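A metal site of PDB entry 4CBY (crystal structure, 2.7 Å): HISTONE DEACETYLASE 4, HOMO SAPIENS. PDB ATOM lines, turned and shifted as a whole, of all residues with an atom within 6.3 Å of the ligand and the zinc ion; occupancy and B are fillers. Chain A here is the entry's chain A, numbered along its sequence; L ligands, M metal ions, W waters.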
ATOM      1  N   PRO A  32      33.059  26.726   9.038  1.00  0.00           N
ATOM      2  CA  PRO A  32      32.769  25.343   8.698  1.00  0.00           C
ATOM      3  C   PRO A  32      33.349  24.891   7.379  1.00  0.00           C
ATOM      4  O   PRO A  32      33.731  23.724   7.252  1.00  0.00           O
ATOM      5  CB  PRO A  32      31.244  25.310   8.611  1.00  0.00           C
ATOM      6  CG  PRO A  32      30.759  26.491   9.382  1.00  0.00           C
ATOM      7  CD  PRO A  32      31.825  27.528   9.217  1.00  0.00           C
ATOM      8  N   GLU A  33      33.427  25.786   6.410  1.00  0.00           N
ATOM      9  CA  GLU A  33      33.991  25.460   5.113  1.00  0.00           C
ATOM     10  C   GLU A  33      35.513  25.665   5.183  1.00  0.00           C
ATOM     11  O   GLU A  33      36.067  26.673   4.741  1.00  0.00           O
ATOM     12  CB  GLU A  33      33.249  26.246   3.995  1.00  0.00           C
ATOM     13  CG  GLU A  33      34.005  26.786   2.782  1.00  0.00           C
ATOM     14  CD  GLU A  33      34.998  25.839   2.125  1.00  0.00           C
ATOM     15  OE1 GLU A  33      34.930  24.608   2.304  1.00  0.00           O
ATOM     16  OE2 GLU A  33      35.860  26.374   1.388  1.00  0.00           O
ATOM     17  N   HIS A  34      36.195  24.661   5.737  1.00  0.00           N
ATOM     18  CA  HIS A  34      37.631  24.781   6.027  1.00  0.00           C
ATOM     19  C   HIS A  34      38.535  23.906   5.201  1.00  0.00           C
ATOM     20  O   HIS A  34      38.120  22.889   4.682  1.00  0.00           O
ATOM     21  CB  HIS A  34      37.879  24.541   7.504  1.00  0.00           C
ATOM     22  CG  HIS A  34      37.516  23.174   7.972  1.00  0.00           C
ATOM     23  ND1 HIS A  34      38.281  22.036   8.156  1.00  0.00           N
ATOM     24  CD2 HIS A  34      36.264  22.859   8.326  1.00  0.00           C
ATOM     25  CE1 HIS A  34      37.474  21.081   8.618  1.00  0.00           C
ATOM     26  NE2 HIS A  34      36.233  21.576   8.700  1.00  0.00           N
ATOM     27  N   ARG A  37      38.751  19.914   4.942  1.00  0.00           N
ATOM     28  CA  ARG A  37      37.728  19.170   4.198  1.00  0.00           C
ATOM     29  C   ARG A  37      38.327  18.411   3.020  1.00  0.00           C
ATOM     30  O   ARG A  37      38.114  17.207   2.884  1.00  0.00           O
ATOM     31  CB  ARG A  37      36.621  20.108   3.737  1.00  0.00           C
ATOM     32  CG  ARG A  37      35.789  20.669   4.884  1.00  0.00           C
ATOM     33  CD  ARG A  37      34.443  21.284   4.462  1.00  0.00           C
ATOM     34  NE  ARG A  37      34.465  21.825   3.107  1.00  0.00           N
ATOM     35  CZ  ARG A  37      33.638  21.468   2.124  1.00  0.00           C
ATOM     36  NH1 ARG A  37      32.668  20.593   2.328  1.00  0.00           N
ATOM     37  NH2 ARG A  37      33.781  22.015   0.925  1.00  0.00           N
ATOM     38  N   ASP A 115      28.116  36.318   6.925  1.00  0.00           N
ATOM     39  CA  ASP A 115      28.587  34.943   7.042  1.00  0.00           C
ATOM     40  C   ASP A 115      29.901  34.691   6.308  1.00  0.00           C
ATOM     41  O   ASP A 115      30.773  33.982   6.809  1.00  0.00           O
ATOM     42  CB  ASP A 115      27.516  33.966   6.530  1.00  0.00           C
ATOM     43  N   PRO A 156      33.200  25.902  -2.434  1.00  0.00           N
ATOM     44  CA  PRO A 156      32.051  25.437  -3.198  1.00  0.00           C
ATOM     45  C   PRO A 156      31.444  26.505  -4.112  1.00  0.00           C
ATOM     46  O   PRO A 156      31.825  27.685  -4.029  1.00  0.00           O
ATOM     47  CB  PRO A 156      31.060  25.017  -2.109  1.00  0.00           C
ATOM     48  CG  PRO A 156      31.359  25.969  -0.986  1.00  0.00           C
ATOM     49  CD  PRO A 156      32.848  26.165  -1.028  1.00  0.00           C
ATOM     50  N   HIS A 158      27.692  26.256  -5.805  1.00  0.00           N
ATOM     51  CA  HIS A 158      26.308  26.281  -6.290  1.00  0.00           C
ATOM     52  C   HIS A 158      25.384  27.366  -5.750  1.00  0.00           C
ATOM     53  O   HIS A 158      24.234  27.487  -6.194  1.00  0.00           O
ATOM     54  CB  HIS A 158      25.702  24.880  -6.194  1.00  0.00           C
ATOM     55  CG  HIS A 158      25.351  24.433  -4.792  1.00  0.00           C
ATOM     56  ND1 HIS A 158      24.286  23.642  -4.535  1.00  0.00           N
ATOM     57  CD2 HIS A 158      25.946  24.693  -3.565  1.00  0.00           C
ATOM     58  CE1 HIS A 158      24.207  23.413  -3.211  1.00  0.00           C
ATOM     59  NE2 HIS A 158      25.224  24.056  -2.621  1.00  0.00           N
ATOM     60  N   HIS A 159      25.854  28.172  -4.806  1.00  0.00           N
ATOM     61  CA  HIS A 159      25.052  29.286  -4.276  1.00  0.00           C
ATOM     62  C   HIS A 159      25.439  30.604  -4.874  1.00  0.00           C
ATOM     63  O   HIS A 159      24.740  31.602  -4.671  1.00  0.00           O
ATOM     64  CB  HIS A 159      25.249  29.388  -2.774  1.00  0.00           C
ATOM     65  CG  HIS A 159      24.675  28.238  -2.011  1.00  0.00           C
ATOM     66  ND1 HIS A 159      23.372  27.956  -2.016  1.00  0.00           N
ATOM     67  CD2 HIS A 159      25.276  27.319  -1.173  1.00  0.00           C
ATOM     68  CE1 HIS A 159      23.138  26.888  -1.218  1.00  0.00           C
ATOM     69  NE2 HIS A 159      24.318  26.499  -0.704  1.00  0.00           N
ATOM     70  N   GLY A 167      26.633  31.706   0.957  1.00  0.00           N
ATOM     71  CA  GLY A 167      26.808  30.310   1.371  1.00  0.00           C
ATOM     72  C   GLY A 167      28.236  29.813   1.181  1.00  0.00           C
ATOM     73  O   GLY A 167      28.453  28.682   0.782  1.00  0.00           O
ATOM     74  N   PHE A 168      29.189  30.698   1.432  1.00  0.00           N
ATOM     75  CA  PHE A 168      30.612  30.399   1.310  1.00  0.00           C
ATOM     76  C   PHE A 168      31.055  30.103  -0.123  1.00  0.00           C
ATOM     77  O   PHE A 168      32.137  29.561  -0.349  1.00  0.00           O
ATOM     78  CB  PHE A 168      31.031  29.249   2.250  1.00  0.00           C
ATOM     79  CG  PHE A 168      30.504  29.395   3.669  1.00  0.00           C
ATOM     80  CD1 PHE A 168      30.389  30.637   4.270  1.00  0.00           C
ATOM     81  CD2 PHE A 168      30.165  28.277   4.407  1.00  0.00           C
ATOM     82  CE1 PHE A 168      29.912  30.758   5.571  1.00  0.00           C
ATOM     83  CE2 PHE A 168      29.693  28.390   5.697  1.00  0.00           C
ATOM     84  CZ  PHE A 168      29.561  29.629   6.283  1.00  0.00           C
ATOM     85  N   CYS A 169      30.220  30.505  -1.086  1.00  0.00           N
ATOM     86  CA  CYS A 169      30.516  30.348  -2.502  1.00  0.00           C
ATOM     87  C   CYS A 169      30.805  31.696  -3.141  1.00  0.00           C
ATOM     88  O   CYS A 169      30.168  32.701  -2.791  1.00  0.00           O
ATOM     89  CB  CYS A 169      29.345  29.706  -3.213  1.00  0.00           C
ATOM     90  SG  CYS A 169      28.889  28.093  -2.581  1.00  0.00           S
ATOM     91  N   ASP A 196      23.537  17.789  -3.119  1.00  0.00           N
ATOM     92  CA  ASP A 196      23.826  18.504  -1.874  1.00  0.00           C
ATOM     93  C   ASP A 196      22.495  18.770  -1.187  1.00  0.00           C
ATOM     94  O   ASP A 196      21.499  19.061  -1.872  1.00  0.00           O
ATOM     95  CB  ASP A 196      24.555  19.824  -2.144  1.00  0.00           C
ATOM     96  CG  ASP A 196      24.905  20.603  -0.860  1.00  0.00           C
ATOM     97  OD1 ASP A 196      24.011  21.220  -0.243  1.00  0.00           O
ATOM     98  OD2 ASP A 196      26.094  20.632  -0.489  1.00  0.00           O
ATOM     99  N   VAL A 197      22.468  18.679   0.135  1.00  0.00           N
ATOM    100  CA  VAL A 197      21.235  18.848   0.893  1.00  0.00           C
ATOM    101  C   VAL A 197      20.626  20.246   0.723  1.00  0.00           C
ATOM    102  O   VAL A 197      19.413  20.394   0.924  1.00  0.00           O
ATOM    103  CB  VAL A 197      21.445  18.562   2.396  1.00  0.00           C
ATOM    104  CG1 VAL A 197      22.195  19.715   3.058  1.00  0.00           C
ATOM    105  CG2 VAL A 197      20.098  18.248   3.089  1.00  0.00           C
ATOM    106  N   HIS A 198      21.429  21.243   0.351  1.00  0.00           N
ATOM    107  CA  HIS A 198      20.923  22.606   0.113  1.00  0.00           C
ATOM    108  C   HIS A 198      20.644  22.867  -1.347  1.00  0.00           C
ATOM    109  O   HIS A 198      21.319  22.314  -2.236  1.00  0.00           O
ATOM    110  CB  HIS A 198      21.919  23.665   0.622  1.00  0.00           C
ATOM    111  CG  HIS A 198      22.276  23.507   2.073  1.00  0.00           C
ATOM    112  ND1 HIS A 198      23.350  22.804   2.468  1.00  0.00           N
ATOM    113  CD2 HIS A 198      21.678  23.981   3.235  1.00  0.00           C
ATOM    114  CE1 HIS A 198      23.439  22.815   3.798  1.00  0.00           C
ATOM    115  NE2 HIS A 198      22.409  23.528   4.280  1.00  0.00           N
ATOM    116  N   HIS A 199      19.639  23.704  -1.620  1.00  0.00           N
ATOM    117  CA  HIS A 199      19.268  24.040  -3.001  1.00  0.00           C
ATOM    118  C   HIS A 199      20.353  24.820  -3.653  1.00  0.00           C
ATOM    119  O   HIS A 199      20.961  25.677  -3.019  1.00  0.00           O
ATOM    120  CB  HIS A 199      17.963  24.845  -3.017  1.00  0.00           C
ATOM    121  CG  HIS A 199      17.488  25.231  -4.408  1.00  0.00           C
ATOM    122  ND1 HIS A 199      17.350  26.515  -4.789  1.00  0.00           N
ATOM    123  CD2 HIS A 199      17.119  24.458  -5.508  1.00  0.00           C
ATOM    124  CE1 HIS A 199      16.937  26.549  -6.052  1.00  0.00           C
ATOM    125  NE2 HIS A 199      16.775  25.299  -6.486  1.00  0.00           N
ATOM    126  N   PHE A 227      17.891  26.922   4.579  1.00  0.00           N
ATOM    127  CA  PHE A 227      18.816  27.677   3.738  1.00  0.00           C
ATOM    128  C   PHE A 227      18.919  26.997   2.371  1.00  0.00           C
ATOM    129  O   PHE A 227      18.969  25.770   2.292  1.00  0.00           O
ATOM    130  CB  PHE A 227      20.187  27.773   4.400  1.00  0.00           C
ATOM    131  CG  PHE A 227      21.176  28.558   3.623  1.00  0.00           C
ATOM    132  CD1 PHE A 227      21.205  29.936   3.694  1.00  0.00           C
ATOM    133  CD2 PHE A 227      22.083  27.915   2.787  1.00  0.00           C
ATOM    134  CE1 PHE A 227      22.108  30.667   2.944  1.00  0.00           C
ATOM    135  CE2 PHE A 227      23.002  28.630   2.038  1.00  0.00           C
ATOM    136  CZ  PHE A 227      23.026  30.012   2.132  1.00  0.00           C
ATOM    137  N   GLY A 288      27.436  17.468  -3.135  1.00  0.00           N
ATOM    138  CA  GLY A 288      27.572  17.810  -1.725  1.00  0.00           C
ATOM    139  C   GLY A 288      27.188  16.611  -0.884  1.00  0.00           C
ATOM    140  O   GLY A 288      26.288  15.857  -1.253  1.00  0.00           O
ATOM    141  N   ASP A 290      26.379  16.815   2.547  1.00  0.00           N
ATOM    142  CA  ASP A 290      25.771  17.228   3.825  1.00  0.00           C
ATOM    143  C   ASP A 290      24.465  16.534   4.160  1.00  0.00           C
ATOM    144  O   ASP A 290      23.945  16.720   5.262  1.00  0.00           O
ATOM    145  CB  ASP A 290      25.603  18.749   3.933  1.00  0.00           C
ATOM    146  CG  ASP A 290      25.280  19.417   2.631  1.00  0.00           C
ATOM    147  OD1 ASP A 290      24.864  18.751   1.647  1.00  0.00           O
ATOM    148  OD2 ASP A 290      25.477  20.650   2.606  1.00  0.00           O
ATOM    149  N   PRO A 298      20.814  22.698  11.745  1.00  0.00           N
ATOM    150  CA  PRO A 298      21.080  23.893  10.935  1.00  0.00           C
ATOM    151  C   PRO A 298      21.733  23.568   9.586  1.00  0.00           C
ATOM    152  O   PRO A 298      21.322  24.097   8.552  1.00  0.00           O
ATOM    153  CB  PRO A 298      22.040  24.698  11.811  1.00  0.00           C
ATOM    154  CG  PRO A 298      21.854  24.153  13.195  1.00  0.00           C
ATOM    155  CD  PRO A 298      21.559  22.703  13.005  1.00  0.00           C
ATOM    156  N   LEU A 299      22.724  22.687   9.612  1.00  0.00           N
ATOM    157  CA  LEU A 299      23.545  22.388   8.436  1.00  0.00           C
ATOM    158  C   LEU A 299      22.911  21.311   7.557  1.00  0.00           C
ATOM    159  O   LEU A 299      23.072  21.316   6.343  1.00  0.00           O
ATOM    160  CB  LEU A 299      24.945  21.963   8.903  1.00  0.00           C
ATOM    161  CG  LEU A 299      26.249  22.211   8.116  1.00  0.00           C
ATOM    162  CD1 LEU A 299      26.660  23.691   8.133  1.00  0.00           C
ATOM    163  CD2 LEU A 299      27.360  21.355   8.717  1.00  0.00           C
ATOM    164  N   GLU A 329      30.683  20.060  -3.422  1.00  0.00           N
ATOM    165  CA  GLU A 329      30.017  21.266  -2.971  1.00  0.00           C
ATOM    166  C   GLU A 329      30.092  21.257  -1.435  1.00  0.00           C
ATOM    167  O   GLU A 329      31.198  21.403  -0.888  1.00  0.00           O
ATOM    168  CB  GLU A 329      28.581  21.346  -3.492  1.00  0.00           C
ATOM    169  CG  GLU A 329      28.447  21.440  -5.015  1.00  0.00           C
ATOM    170  CD  GLU A 329      28.750  22.815  -5.601  1.00  0.00           C
ATOM    171  OE1 GLU A 329      29.054  23.755  -4.843  1.00  0.00           O
ATOM    172  OE2 GLU A 329      28.706  22.952  -6.841  1.00  0.00           O
ATOM    173  N   GLY A 330      28.973  21.044  -0.736  1.00  0.00           N
ATOM    174  CA  GLY A 330      28.954  21.013   0.733  1.00  0.00           C
ATOM    175  C   GLY A 330      29.348  19.666   1.346  1.00  0.00           C
ATOM    176  O   GLY A 330      29.818  18.760   0.648  1.00  0.00           O
ATOM    177  N   GLY A 331      29.160  19.568   2.673  1.00  0.00           N
ATOM    178  CA  GLY A 331      29.560  18.395   3.443  1.00  0.00           C
ATOM    179  C   GLY A 331      30.684  18.698   4.409  1.00  0.00           C
ATOM    180  O   GLY A 331      31.786  19.025   3.975  1.00  0.00           O
ATOM    181  N   HIS A 332      30.413  18.601   5.714  1.00  0.00           N
ATOM    182  CA  HIS A 332      31.293  19.131   6.773  1.00  0.00           C
ATOM    183  C   HIS A 332      31.981  18.067   7.553  1.00  0.00           C
ATOM    184  O   HIS A 332      33.198  18.086   7.738  1.00  0.00           O
ATOM    185  CB  HIS A 332      30.466  20.015   7.715  1.00  0.00           C
ATOM    186  CG  HIS A 332      31.207  20.470   8.941  1.00  0.00           C
ATOM    187  ND1 HIS A 332      31.864  21.649   9.005  1.00  0.00           N
ATOM    188  CD2 HIS A 332      31.345  19.891  10.193  1.00  0.00           C
ATOM    189  CE1 HIS A 332      32.404  21.791  10.226  1.00  0.00           C
ATOM    190  NE2 HIS A 332      32.090  20.714  10.945  1.00  0.00           N
HETATM  191  C1  LIG L   1      26.098  24.267   2.118  1.00  0.00           C
HETATM  192  C2  LIG L   1      26.246  25.562   2.907  1.00  0.00           C
HETATM  193  C3  LIG L   1      26.376  25.647   4.447  1.00  0.00           C
HETATM  194  C4  LIG L   1      27.594  25.891   3.546  1.00  0.00           C
HETATM  195  C5  LIG L   1      25.618  26.808   5.019  1.00  0.00           C
HETATM  196  C6  LIG L   1      24.406  26.488   5.630  1.00  0.00           C
HETATM  197  C7  LIG L   1      23.602  27.453   6.193  1.00  0.00           C
HETATM  198  C8  LIG L   1      23.991  28.784   6.169  1.00  0.00           C
HETATM  199  C9  LIG L   1      25.193  29.137   5.547  1.00  0.00           C
HETATM  200  C10 LIG L   1      26.018  28.147   4.974  1.00  0.00           C
HETATM  201  C11 LIG L   1      28.682  24.910   3.740  1.00  0.00           C
HETATM  202  C12 LIG L   1      29.407  24.458   2.640  1.00  0.00           C
HETATM  203  C13 LIG L   1      30.458  23.570   2.832  1.00  0.00           C
HETATM  204  C14 LIG L   1      30.805  23.136   4.113  1.00  0.00           C
HETATM  205  C15 LIG L   1      30.095  23.621   5.215  1.00  0.00           C
HETATM  206  C16 LIG L   1      29.044  24.508   5.024  1.00  0.00           C
HETATM  207  C17 LIG L   1      23.061  29.769   6.779  1.00  0.00           C
HETATM  208  O1  LIG L   1      22.735  31.005   6.280  1.00  0.00           O
HETATM  209  C18 LIG L   1      21.803  31.582   7.134  1.00  0.00           C
HETATM  210  N1  LIG L   1      21.559  30.699   8.137  1.00  0.00           N
HETATM  211  C19 LIG L   1      22.306  29.582   7.941  1.00  0.00           C
HETATM  212  O2  LIG L   1      26.122  23.115   2.563  1.00  0.00           O
HETATM  213  N2  LIG L   1      25.873  24.545   0.839  1.00  0.00           N
HETATM  214  O3  LIG L   1      25.590  23.559  -0.109  1.00  0.00           O
HETATM  215 ZN    ZN M   1      24.976  22.050   1.331  1.00  0.00          ZN
HETATM  216  O   HOH W   1      27.266  21.316   4.662  1.00  0.00           O
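A ring nitrogen (NE2) of His 158 sits close to an oxygen (O3) of the ligand, 2.6 Å away.
A nitrogen (N2) of the ligand is in hydrogen-bond range of a ring nitrogen (NE2) of His 159 (2.9 Å).
OD1 of Asp 290 lies within hydrogen-bond range of N of Val 197 (2.8 Å).
OD2 of Asp 196 lies close to N of Gly 330.
NE2 of His 198 sits close to O of Leu 299, 3.1 Å away.
NE2 of His 159 lies within hydrogen-bond range of NE2 of His 158.
N of His 158 is in hydrogen-bond range of OE1 of Glu 329 (3.0 Å).
The backbone NH (N) of His 159 lies within hydrogen-bond range of the side-chain sulfur (SG) of Cys 169 (3.8 Å).
A ring nitrogen (ND1) of His 159 lies close to the backbone carbonyl oxygen of His 199 (3.5 Å).
The guanidinium group (NH1) of Arg 37 is in hydrogen-bond range of the backbone carbonyl oxygen (O) of Gly 331, at 2.4 Å.
Merely in contact with the ligand: Pro 32, Glu 33, Arg 37, Phe 168, Phe 227 and Gly 330.
Within 4 Å of the ligand: Pro 32, Glu 33, Arg 37, His 158, His 159, Phe 168, Asp 196, His 198, Phe 227, Asp 290 and Gly 330.
Three residues have an atom within 4 Å of the zinc ion: Asp 196, His 198 and Asp 290.
The zinc ion is bound by OD2 of Asp 290 (2.0 Å), O2 of the ligand (2.0 Å), OD1 of Asp 196 (2.0 Å), ND1 of His 198 (2.1 Å), O3 of the ligand (2.2 Å) and OD2 of Asp 196 (2.6 Å).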
